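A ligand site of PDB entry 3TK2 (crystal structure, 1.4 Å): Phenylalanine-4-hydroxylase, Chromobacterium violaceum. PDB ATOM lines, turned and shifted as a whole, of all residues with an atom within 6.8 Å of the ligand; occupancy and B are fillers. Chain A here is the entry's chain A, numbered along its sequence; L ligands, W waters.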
ATOM      1  N   ASP A 159     -20.876  -9.162  -0.115  1.00  0.00           N
ATOM      2  CA  ASP A 159     -21.182  -8.665  -1.477  1.00  0.00           C
ATOM      3  C   ASP A 159     -22.529  -7.971  -1.488  1.00  0.00           C
ATOM      4  O   ASP A 159     -22.693  -6.998  -2.186  1.00  0.00           O
ATOM      5  CB  ASP A 159     -21.224  -9.841  -2.432  1.00  0.00           C
ATOM      6  CG  ASP A 159     -19.849 -10.278  -2.901  1.00  0.00           C
ATOM      7  OD1 ASP A 159     -18.834  -9.574  -2.634  1.00  0.00           O
ATOM      8  OD2 ASP A 159     -19.798 -11.367  -3.521  1.00  0.00           O
ATOM      9  N   TYR A 160     -23.507  -8.456  -0.686  1.00  0.00           N
ATOM     10  CA  TYR A 160     -24.755  -7.728  -0.586  1.00  0.00           C
ATOM     11  C   TYR A 160     -24.554  -6.273  -0.081  1.00  0.00           C
ATOM     12  O   TYR A 160     -25.094  -5.337  -0.638  1.00  0.00           O
ATOM     13  CB  TYR A 160     -25.712  -8.461   0.343  1.00  0.00           C
ATOM     14  CG  TYR A 160     -26.976  -7.742   0.721  1.00  0.00           C
ATOM     15  CD1 TYR A 160     -27.901  -7.347  -0.223  1.00  0.00           C
ATOM     16  CD2 TYR A 160     -27.215  -7.447   2.062  1.00  0.00           C
ATOM     17  CE1 TYR A 160     -29.050  -6.686   0.124  1.00  0.00           C
ATOM     18  CE2 TYR A 160     -28.417  -6.746   2.405  1.00  0.00           C
ATOM     19  CZ  TYR A 160     -29.306  -6.384   1.424  1.00  0.00           C
ATOM     20  OH  TYR A 160     -30.467  -5.760   1.717  1.00  0.00           O
ATOM     21  N   LEU A 161     -23.725  -6.121   0.955  1.00  0.00           N
ATOM     22  CA  LEU A 161     -23.477  -4.766   1.491  1.00  0.00           C
ATOM     23  C   LEU A 161     -22.779  -3.879   0.491  1.00  0.00           C
ATOM     24  O   LEU A 161     -23.092  -2.696   0.397  1.00  0.00           O
ATOM     25  CB  LEU A 161     -22.701  -4.794   2.780  1.00  0.00           C
ATOM     26  CG  LEU A 161     -23.391  -5.239   4.003  1.00  0.00           C
ATOM     27  CD1 LEU A 161     -22.416  -5.129   5.144  1.00  0.00           C
ATOM     28  CD2 LEU A 161     -24.587  -4.377   4.271  1.00  0.00           C
ATOM     29  N   GLU A 162     -21.791  -4.429  -0.229  1.00  0.00           N
ATOM     30  CA  GLU A 162     -21.136  -3.643  -1.225  1.00  0.00           C
ATOM     31  C   GLU A 162     -22.086  -3.217  -2.327  1.00  0.00           C
ATOM     32  O   GLU A 162     -22.082  -2.069  -2.775  1.00  0.00           O
ATOM     33  CB  GLU A 162     -19.940  -4.449  -1.828  1.00  0.00           C
ATOM     34  CG  GLU A 162     -19.212  -3.724  -2.915  1.00  0.00           C
ATOM     35  CD  GLU A 162     -18.095  -4.520  -3.544  1.00  0.00           C
ATOM     36  OE1 GLU A 162     -17.748  -5.616  -3.114  1.00  0.00           O
ATOM     37  OE2 GLU A 162     -17.565  -3.997  -4.536  1.00  0.00           O
ATOM     38  N   ALA A 163     -22.932  -4.149  -2.764  1.00  0.00           N
ATOM     39  CA  ALA A 163     -23.922  -3.828  -3.788  1.00  0.00           C
ATOM     40  C   ALA A 163     -24.880  -2.769  -3.324  1.00  0.00           C
ATOM     41  O   ALA A 163     -25.287  -1.855  -4.077  1.00  0.00           O
ATOM     42  CB  ALA A 163     -24.648  -5.100  -4.257  1.00  0.00           C
ATOM     43  N   TYR A 164     -25.332  -2.892  -2.078  1.00  0.00           N
ATOM     44  CA  TYR A 164     -26.217  -1.902  -1.474  1.00  0.00           C
ATOM     45  C   TYR A 164     -25.507  -0.536  -1.521  1.00  0.00           C
ATOM     46  O   TYR A 164     -26.120   0.509  -1.916  1.00  0.00           O
ATOM     47  CB  TYR A 164     -26.522  -2.343  -0.009  1.00  0.00           C
ATOM     48  CG  TYR A 164     -27.336  -1.316   0.735  1.00  0.00           C
ATOM     49  CD1 TYR A 164     -28.735  -1.291   0.676  1.00  0.00           C
ATOM     50  CD2 TYR A 164     -26.718  -0.321   1.442  1.00  0.00           C
ATOM     51  CE1 TYR A 164     -29.484  -0.333   1.300  1.00  0.00           C
ATOM     52  CE2 TYR A 164     -27.475   0.677   2.107  1.00  0.00           C
ATOM     53  CZ  TYR A 164     -28.872   0.636   2.033  1.00  0.00           C
ATOM     54  OH  TYR A 164     -29.643   1.576   2.641  1.00  0.00           O
ATOM     55  N   GLY A 165     -24.256  -0.461  -1.058  1.00  0.00           N
ATOM     56  CA  GLY A 165     -23.490   0.782  -1.097  1.00  0.00           C
ATOM     57  C   GLY A 165     -23.481   1.403  -2.492  1.00  0.00           C
ATOM     58  O   GLY A 165     -23.768   2.602  -2.672  1.00  0.00           O
ATOM     59  N   LYS A 166     -23.202   0.590  -3.494  1.00  0.00           N
ATOM     60  CA  LYS A 166     -23.120   1.065  -4.859  1.00  0.00           C
ATOM     61  C   LYS A 166     -24.469   1.595  -5.338  1.00  0.00           C
ATOM     62  O   LYS A 166     -24.471   2.464  -6.209  1.00  0.00           O
ATOM     63  CB  LYS A 166     -22.624  -0.123  -5.719  1.00  0.00           C
ATOM     64  CG  LYS A 166     -21.174  -0.361  -5.541  1.00  0.00           C
ATOM     65  CD  LYS A 166     -20.710  -1.582  -6.343  1.00  0.00           C
ATOM     66  CE  LYS A 166     -19.237  -1.605  -6.247  1.00  0.00           C
ATOM     67  NZ  LYS A 166     -18.514  -2.784  -6.899  1.00  0.00           N
ATOM     68  N   GLY A 167     -25.581   1.069  -4.821  1.00  0.00           N
ATOM     69  CA  GLY A 167     -26.909   1.611  -5.180  1.00  0.00           C
ATOM     70  C   GLY A 167     -27.230   2.999  -4.625  1.00  0.00           C
ATOM     71  O   GLY A 167     -28.234   3.578  -5.040  1.00  0.00           O
ATOM     72  N   GLY A 168     -26.437   3.539  -3.732  1.00  0.00           N
ATOM     73  CA  GLY A 168     -26.789   4.822  -3.155  1.00  0.00           C
ATOM     74  C   GLY A 168     -26.785   5.930  -4.168  1.00  0.00           C
ATOM     75  O   GLY A 168     -27.523   6.885  -4.005  1.00  0.00           O
ATOM     76  N   LYS A 170     -27.625   5.976  -7.440  1.00  0.00           N
ATOM     77  CA  LYS A 170     -28.870   5.975  -8.211  1.00  0.00           C
ATOM     78  C   LYS A 170     -29.991   6.419  -7.299  1.00  0.00           C
ATOM     79  O   LYS A 170     -30.885   7.188  -7.707  1.00  0.00           O
ATOM     80  CB  LYS A 170     -29.130   4.567  -8.783  1.00  0.00           C
ATOM     81  CG  LYS A 170     -30.474   4.383  -9.458  1.00  0.00           C
ATOM     82  CD  LYS A 170     -30.754   2.931  -9.936  1.00  0.00           C
ATOM     83  CE  LYS A 170     -29.730   2.363 -10.940  1.00  0.00           C
ATOM     84  NZ  LYS A 170     -30.192   0.948 -11.295  1.00  0.00           N
ATOM     85  N   ALA A 171     -30.038   5.896  -6.079  1.00  0.00           N
ATOM     86  CA  ALA A 171     -31.123   6.268  -5.190  1.00  0.00           C
ATOM     87  C   ALA A 171     -31.104   7.774  -4.895  1.00  0.00           C
ATOM     88  O   ALA A 171     -32.150   8.409  -4.911  1.00  0.00           O
ATOM     89  CB  ALA A 171     -31.070   5.423  -3.907  1.00  0.00           C
ATOM     90  N   LEU A 180     -34.259   2.810  -0.149  1.00  0.00           N
ATOM     91  CA  LEU A 180     -33.107   1.935   0.224  1.00  0.00           C
ATOM     92  C   LEU A 180     -32.978   1.809   1.697  1.00  0.00           C
ATOM     93  O   LEU A 180     -32.627   0.733   2.169  1.00  0.00           O
ATOM     94  CB  LEU A 180     -31.760   2.322  -0.362  1.00  0.00           C
ATOM     95  CG  LEU A 180     -31.541   2.101  -1.818  1.00  0.00           C
ATOM     96  CD1 LEU A 180     -30.151   2.526  -2.145  1.00  0.00           C
ATOM     97  CD2 LEU A 180     -31.693   0.593  -1.972  1.00  0.00           C
ATOM     98  N   LEU A 183     -35.024  -0.971   2.926  1.00  0.00           N
ATOM     99  CA  LEU A 183     -34.421  -2.283   2.643  1.00  0.00           C
ATOM    100  C   LEU A 183     -33.281  -2.609   3.619  1.00  0.00           C
ATOM    101  O   LEU A 183     -33.217  -3.710   4.167  1.00  0.00           O
ATOM    102  CB  LEU A 183     -33.874  -2.248   1.214  1.00  0.00           C
ATOM    103  CG  LEU A 183     -33.177  -3.552   0.802  1.00  0.00           C
ATOM    104  CD1 LEU A 183     -34.066  -4.832   0.874  1.00  0.00           C
ATOM    105  CD2 LEU A 183     -32.569  -3.379  -0.620  1.00  0.00           C
ATOM    106  N   LEU A 229     -38.813  -7.758  -2.084  1.00  0.00           N
ATOM    107  CA  LEU A 229     -38.109  -6.473  -2.248  1.00  0.00           C
ATOM    108  C   LEU A 229     -39.062  -5.310  -2.356  1.00  0.00           C
ATOM    109  O   LEU A 229     -38.873  -4.286  -1.672  1.00  0.00           O
ATOM    110  CB  LEU A 229     -37.288  -6.560  -3.529  1.00  0.00           C
ATOM    111  CG  LEU A 229     -36.631  -5.248  -3.937  1.00  0.00           C
ATOM    112  CD1 LEU A 229     -35.621  -4.775  -2.838  1.00  0.00           C
ATOM    113  CD2 LEU A 229     -35.929  -5.429  -5.255  1.00  0.00           C
ATOM    114  N   MET A 233     -39.446  -2.126   0.349  1.00  0.00           N
ATOM    115  CA  MET A 233     -39.099  -0.745   0.038  1.00  0.00           C
ATOM    116  C   MET A 233     -40.309   0.153   0.112  1.00  0.00           C
ATOM    117  O   MET A 233     -40.133   1.354   0.059  1.00  0.00           O
ATOM    118  CB  MET A 233     -38.430  -0.612  -1.297  1.00  0.00           C
ATOM    119  CG  MET A 233     -37.026  -1.280  -1.221  1.00  0.00           C
ATOM    120  SD  MET A 233     -35.918  -0.696  -2.589  1.00  0.00           S
ATOM    121  CE  MET A 233     -36.813  -1.260  -4.073  1.00  0.00           C
ATOM    122  N   LEU A 255     -30.805 -12.342  -0.556  1.00  0.00           N
ATOM    123  CA  LEU A 255     -30.582 -10.877  -0.460  1.00  0.00           C
ATOM    124  C   LEU A 255     -29.834 -10.525  -1.638  1.00  0.00           C
ATOM    125  O   LEU A 255     -30.245  -9.623  -2.308  1.00  0.00           O
ATOM    126  CB  LEU A 255     -29.833 -10.335   0.828  1.00  0.00           C
ATOM    127  CG  LEU A 255     -30.362 -10.519   2.188  1.00  0.00           C
ATOM    128  CD1 LEU A 255     -29.364 -10.280   3.191  1.00  0.00           C
ATOM    129  CD2 LEU A 255     -31.537  -9.639   2.295  1.00  0.00           C
ATOM    130  N   PHE A 256     -28.752 -11.257  -1.927  1.00  0.00           N
ATOM    131  CA  PHE A 256     -27.907 -10.782  -2.975  1.00  0.00           C
ATOM    132  C   PHE A 256     -28.652 -10.831  -4.346  1.00  0.00           C
ATOM    133  O   PHE A 256     -28.672  -9.803  -5.061  1.00  0.00           O
ATOM    134  CB  PHE A 256     -26.572 -11.544  -3.021  1.00  0.00           C
ATOM    135  CG  PHE A 256     -25.707 -10.994  -4.073  1.00  0.00           C
ATOM    136  CD1 PHE A 256     -24.948  -9.862  -3.827  1.00  0.00           C
ATOM    137  CD2 PHE A 256     -25.738 -11.533  -5.394  1.00  0.00           C
ATOM    138  CE1 PHE A 256     -24.143  -9.327  -4.808  1.00  0.00           C
ATOM    139  CE2 PHE A 256     -24.933 -10.966  -6.373  1.00  0.00           C
ATOM    140  CZ  PHE A 256     -24.136  -9.831  -6.054  1.00  0.00           C
ATOM    141  N   THR A 259     -32.050  -8.716  -4.887  1.00  0.00           N
ATOM    142  CA  THR A 259     -31.709  -7.331  -4.957  1.00  0.00           C
ATOM    143  C   THR A 259     -30.679  -6.926  -6.004  1.00  0.00           C
ATOM    144  O   THR A 259     -30.269  -5.761  -6.001  1.00  0.00           O
ATOM    145  CB  THR A 259     -31.170  -6.759  -3.550  1.00  0.00           C
ATOM    146  OG1 THR A 259     -29.960  -7.459  -3.192  1.00  0.00           O
ATOM    147  CG2 THR A 259     -32.228  -6.932  -2.429  1.00  0.00           C
ATOM    148  N   ALA A 260     -30.421  -7.767  -7.020  1.00  0.00           N
ATOM    149  CA  ALA A 260     -29.589  -7.390  -8.162  1.00  0.00           C
ATOM    150  C   ALA A 260     -30.232  -6.682  -9.462  1.00  0.00           C
ATOM    151  O   ALA A 260     -29.518  -6.077 -10.255  1.00  0.00           O
ATOM    152  CB  ALA A 260     -28.753  -8.643  -8.687  1.00  0.00           C
ATOM    153  N   PRO A 261     -31.576  -6.764  -9.708  1.00  0.00           N
ATOM    154  CA  PRO A 261     -32.203  -6.031 -10.788  1.00  0.00           C
ATOM    155  C   PRO A 261     -32.110  -4.461 -10.719  1.00  0.00           C
ATOM    156  O   PRO A 261     -31.736  -3.885  -9.693  1.00  0.00           O
ATOM    157  CB  PRO A 261     -33.639  -6.477 -10.688  1.00  0.00           C
ATOM    158  CG  PRO A 261     -33.548  -7.846 -10.059  1.00  0.00           C
ATOM    159  CD  PRO A 261     -32.533  -7.615  -9.013  1.00  0.00           C
ATOM    160  N   ASP A 262     -32.437  -3.778 -11.807  1.00  0.00           N
ATOM    161  CA  ASP A 262     -32.408  -2.299 -11.850  1.00  0.00           C
ATOM    162  C   ASP A 262     -33.493  -1.753 -10.936  1.00  0.00           C
ATOM    163  O   ASP A 262     -34.690  -2.027 -11.136  1.00  0.00           O
ATOM    164  CB  ASP A 262     -32.704  -1.891 -13.326  1.00  0.00           C
ATOM    165  CG  ASP A 262     -32.811  -0.395 -13.498  1.00  0.00           C
ATOM    166  OD1 ASP A 262     -32.451   0.368 -12.556  1.00  0.00           O
ATOM    167  OD2 ASP A 262     -33.306   0.050 -14.574  1.00  0.00           O
ATOM    168  N   PHE A 263     -33.125  -0.991  -9.912  1.00  0.00           N
ATOM    169  CA  PHE A 263     -34.115  -0.462  -8.968  1.00  0.00           C
ATOM    170  C   PHE A 263     -34.811   0.808  -9.491  1.00  0.00           C
ATOM    171  O   PHE A 263     -35.797   1.191  -8.900  1.00  0.00           O
ATOM    172  CB  PHE A 263     -33.475  -0.150  -7.635  1.00  0.00           C
ATOM    173  CG  PHE A 263     -33.252  -1.336  -6.735  1.00  0.00           C
ATOM    174  CD1 PHE A 263     -33.078  -1.101  -5.360  1.00  0.00           C
ATOM    175  CD2 PHE A 263     -33.200  -2.654  -7.221  1.00  0.00           C
ATOM    176  CE1 PHE A 263     -32.844  -2.140  -4.509  1.00  0.00           C
ATOM    177  CE2 PHE A 263     -32.940  -3.716  -6.315  1.00  0.00           C
ATOM    178  CZ  PHE A 263     -32.748  -3.452  -5.002  1.00  0.00           C
ATOM    179  N   ALA A 264     -34.328   1.423 -10.586  1.00  0.00           N
ATOM    180  CA  ALA A 264     -34.906   2.686 -11.010  1.00  0.00           C
ATOM    181  C   ALA A 264     -36.426   2.610 -11.265  1.00  0.00           C
ATOM    182  O   ALA A 264     -37.168   3.452 -10.742  1.00  0.00           O
ATOM    183  CB  ALA A 264     -34.143   3.316 -12.173  1.00  0.00           C
ATOM    184  N   TYR A 267     -38.231   2.306  -7.862  1.00  0.00           N
ATOM    185  CA  TYR A 267     -38.371   3.581  -7.135  1.00  0.00           C
ATOM    186  C   TYR A 267     -39.471   4.431  -7.698  1.00  0.00           C
ATOM    187  O   TYR A 267     -40.231   5.029  -6.910  1.00  0.00           O
ATOM    188  CB  TYR A 267     -37.089   4.336  -7.219  1.00  0.00           C
ATOM    189  CG  TYR A 267     -35.878   3.713  -6.538  1.00  0.00           C
ATOM    190  CD1 TYR A 267     -34.640   3.893  -7.114  1.00  0.00           C
ATOM    191  CD2 TYR A 267     -35.991   2.960  -5.352  1.00  0.00           C
ATOM    192  CE1 TYR A 267     -33.487   3.420  -6.548  1.00  0.00           C
ATOM    193  CE2 TYR A 267     -34.846   2.438  -4.764  1.00  0.00           C
ATOM    194  CZ  TYR A 267     -33.606   2.664  -5.370  1.00  0.00           C
ATOM    195  OH  TYR A 267     -32.458   2.139  -4.795  1.00  0.00           O
HETATM  196  N1  LIG L   1     -29.887  -3.341  -7.775  1.00  0.00           N
HETATM  197  C1  LIG L   1     -29.880  -2.014  -7.079  1.00  0.00           C
HETATM  198  C2  LIG L   1     -29.888  -0.903  -8.111  1.00  0.00           C
HETATM  199  O1  LIG L   1     -29.534   0.258  -7.817  1.00  0.00           O
HETATM  200  C3  LIG L   1     -28.632  -1.795  -6.225  1.00  0.00           C
HETATM  201  C4  LIG L   1     -28.730  -2.483  -4.910  1.00  0.00           C
HETATM  202  C5  LIG L   1     -28.076  -3.723  -4.710  1.00  0.00           C
HETATM  203  C6  LIG L   1     -29.525  -1.893  -3.907  1.00  0.00           C
HETATM  204  C7  LIG L   1     -28.214  -4.399  -3.487  1.00  0.00           C
HETATM  205  C8  LIG L   1     -29.662  -2.600  -2.684  1.00  0.00           C
HETATM  206  C9  LIG L   1     -29.011  -3.837  -2.471  1.00  0.00           C
HETATM  207  O2  LIG L   1     -30.230  -1.130  -9.235  1.00  0.00           O
HETATM  208  O   HOH W   1     -27.189  -4.071  -8.591  1.00  0.00           O
HETATM  209  O   HOH W   2     -27.395   1.201  -8.890  1.00  0.00           O
HETATM  210  O   HOH W   3     -28.707  -2.006 -12.016  1.00  0.00           O
HETATM  211  O   HOH W   4     -30.273   2.210  -6.276  1.00  0.00           O
HETATM  212  O   HOH W   5     -27.535  -7.399  -5.083  1.00  0.00           O
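N1 of the ligand lies within hydrogen-bond range of O of Pro 261 (2.7 Å).
The side-chain amino group of Lys 170 is in salt-bridge range of an oxygen (O2) of the ligand (2.9 Å).
An oxygen (O2) of the ligand sits at hydrogen-bond distance from the backbone NH (N) of Phe 263 (3.0 Å).
A nitrogen (N1) of the ligand lies within hydrogen-bond range of the backbone carbonyl oxygen (O) of Thr 259.
The side-chain amino group (NZ) of Lys 170 is in salt-bridge range of the side-chain carboxylate (OD1) of Asp 262, at 2.7 Å.
The side-chain hydroxyl (OG1) of Thr 259 is in hydrogen-bond range of the backbone carbonyl oxygen (O) of Phe 256 (3.3 Å).
The backbone carbonyl oxygen (O) of Leu 180 lies within hydrogen-bond range of the side-chain hydroxyl (OH) of Tyr 164 (3.1 Å).
OD1 of Asp 262 lies within hydrogen-bond range of N of Ala 264 (2.9 Å).
Water W4 lies within hydrogen-bond range of O1 of the ligand (2.6 Å), OH of Tyr 267 (2.6 Å) and O of Gly 167 (2.7 Å).
Water W1 bridges N1 of the ligand (2.9 Å) and O of Ala 260 (3.5 Å).
Water W3 bridges O2 of the ligand (3.3 Å) and NZ of Lys 170 (3.4 Å).
Water W5 lies within hydrogen-bond range of the backbone carbonyl oxygen (O) of Phe 256 (2.7 Å), the side-chain hydroxyl (OG1) of Thr 259 (3.1 Å) and the backbone NH (N) of Ala 260 (3.5 Å).
Tyr 160 touches the ligand (CE1 to C9, 3.9 Å).
O of Ala 163 touches C5 of the ligand, at 3.4 Å.
Tyr 164 touches the ligand (CA to C9, 3.5 Å).
CA of Gly 167 touches C3 of the ligand, 3.96 Å away.
Leu 180 touches the ligand.
Leu 183 touches the ligand.
Ala 260 touches the ligand (O to N1, 3.7 Å).
Asp 262 touches the ligand (CA to O2, 3.6 Å).
Hydrophobic or aromatic side chains within 4 Å of the ligand: Tyr 160, Ala 163, Tyr 164, Leu 180, Leu 183 and Phe 263.
Of the 25 residues printed, 12 come within 4 Å of the ligand.
The nearest printed residue that does not touch the ligand is Tyr 267 (4.6 Å).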
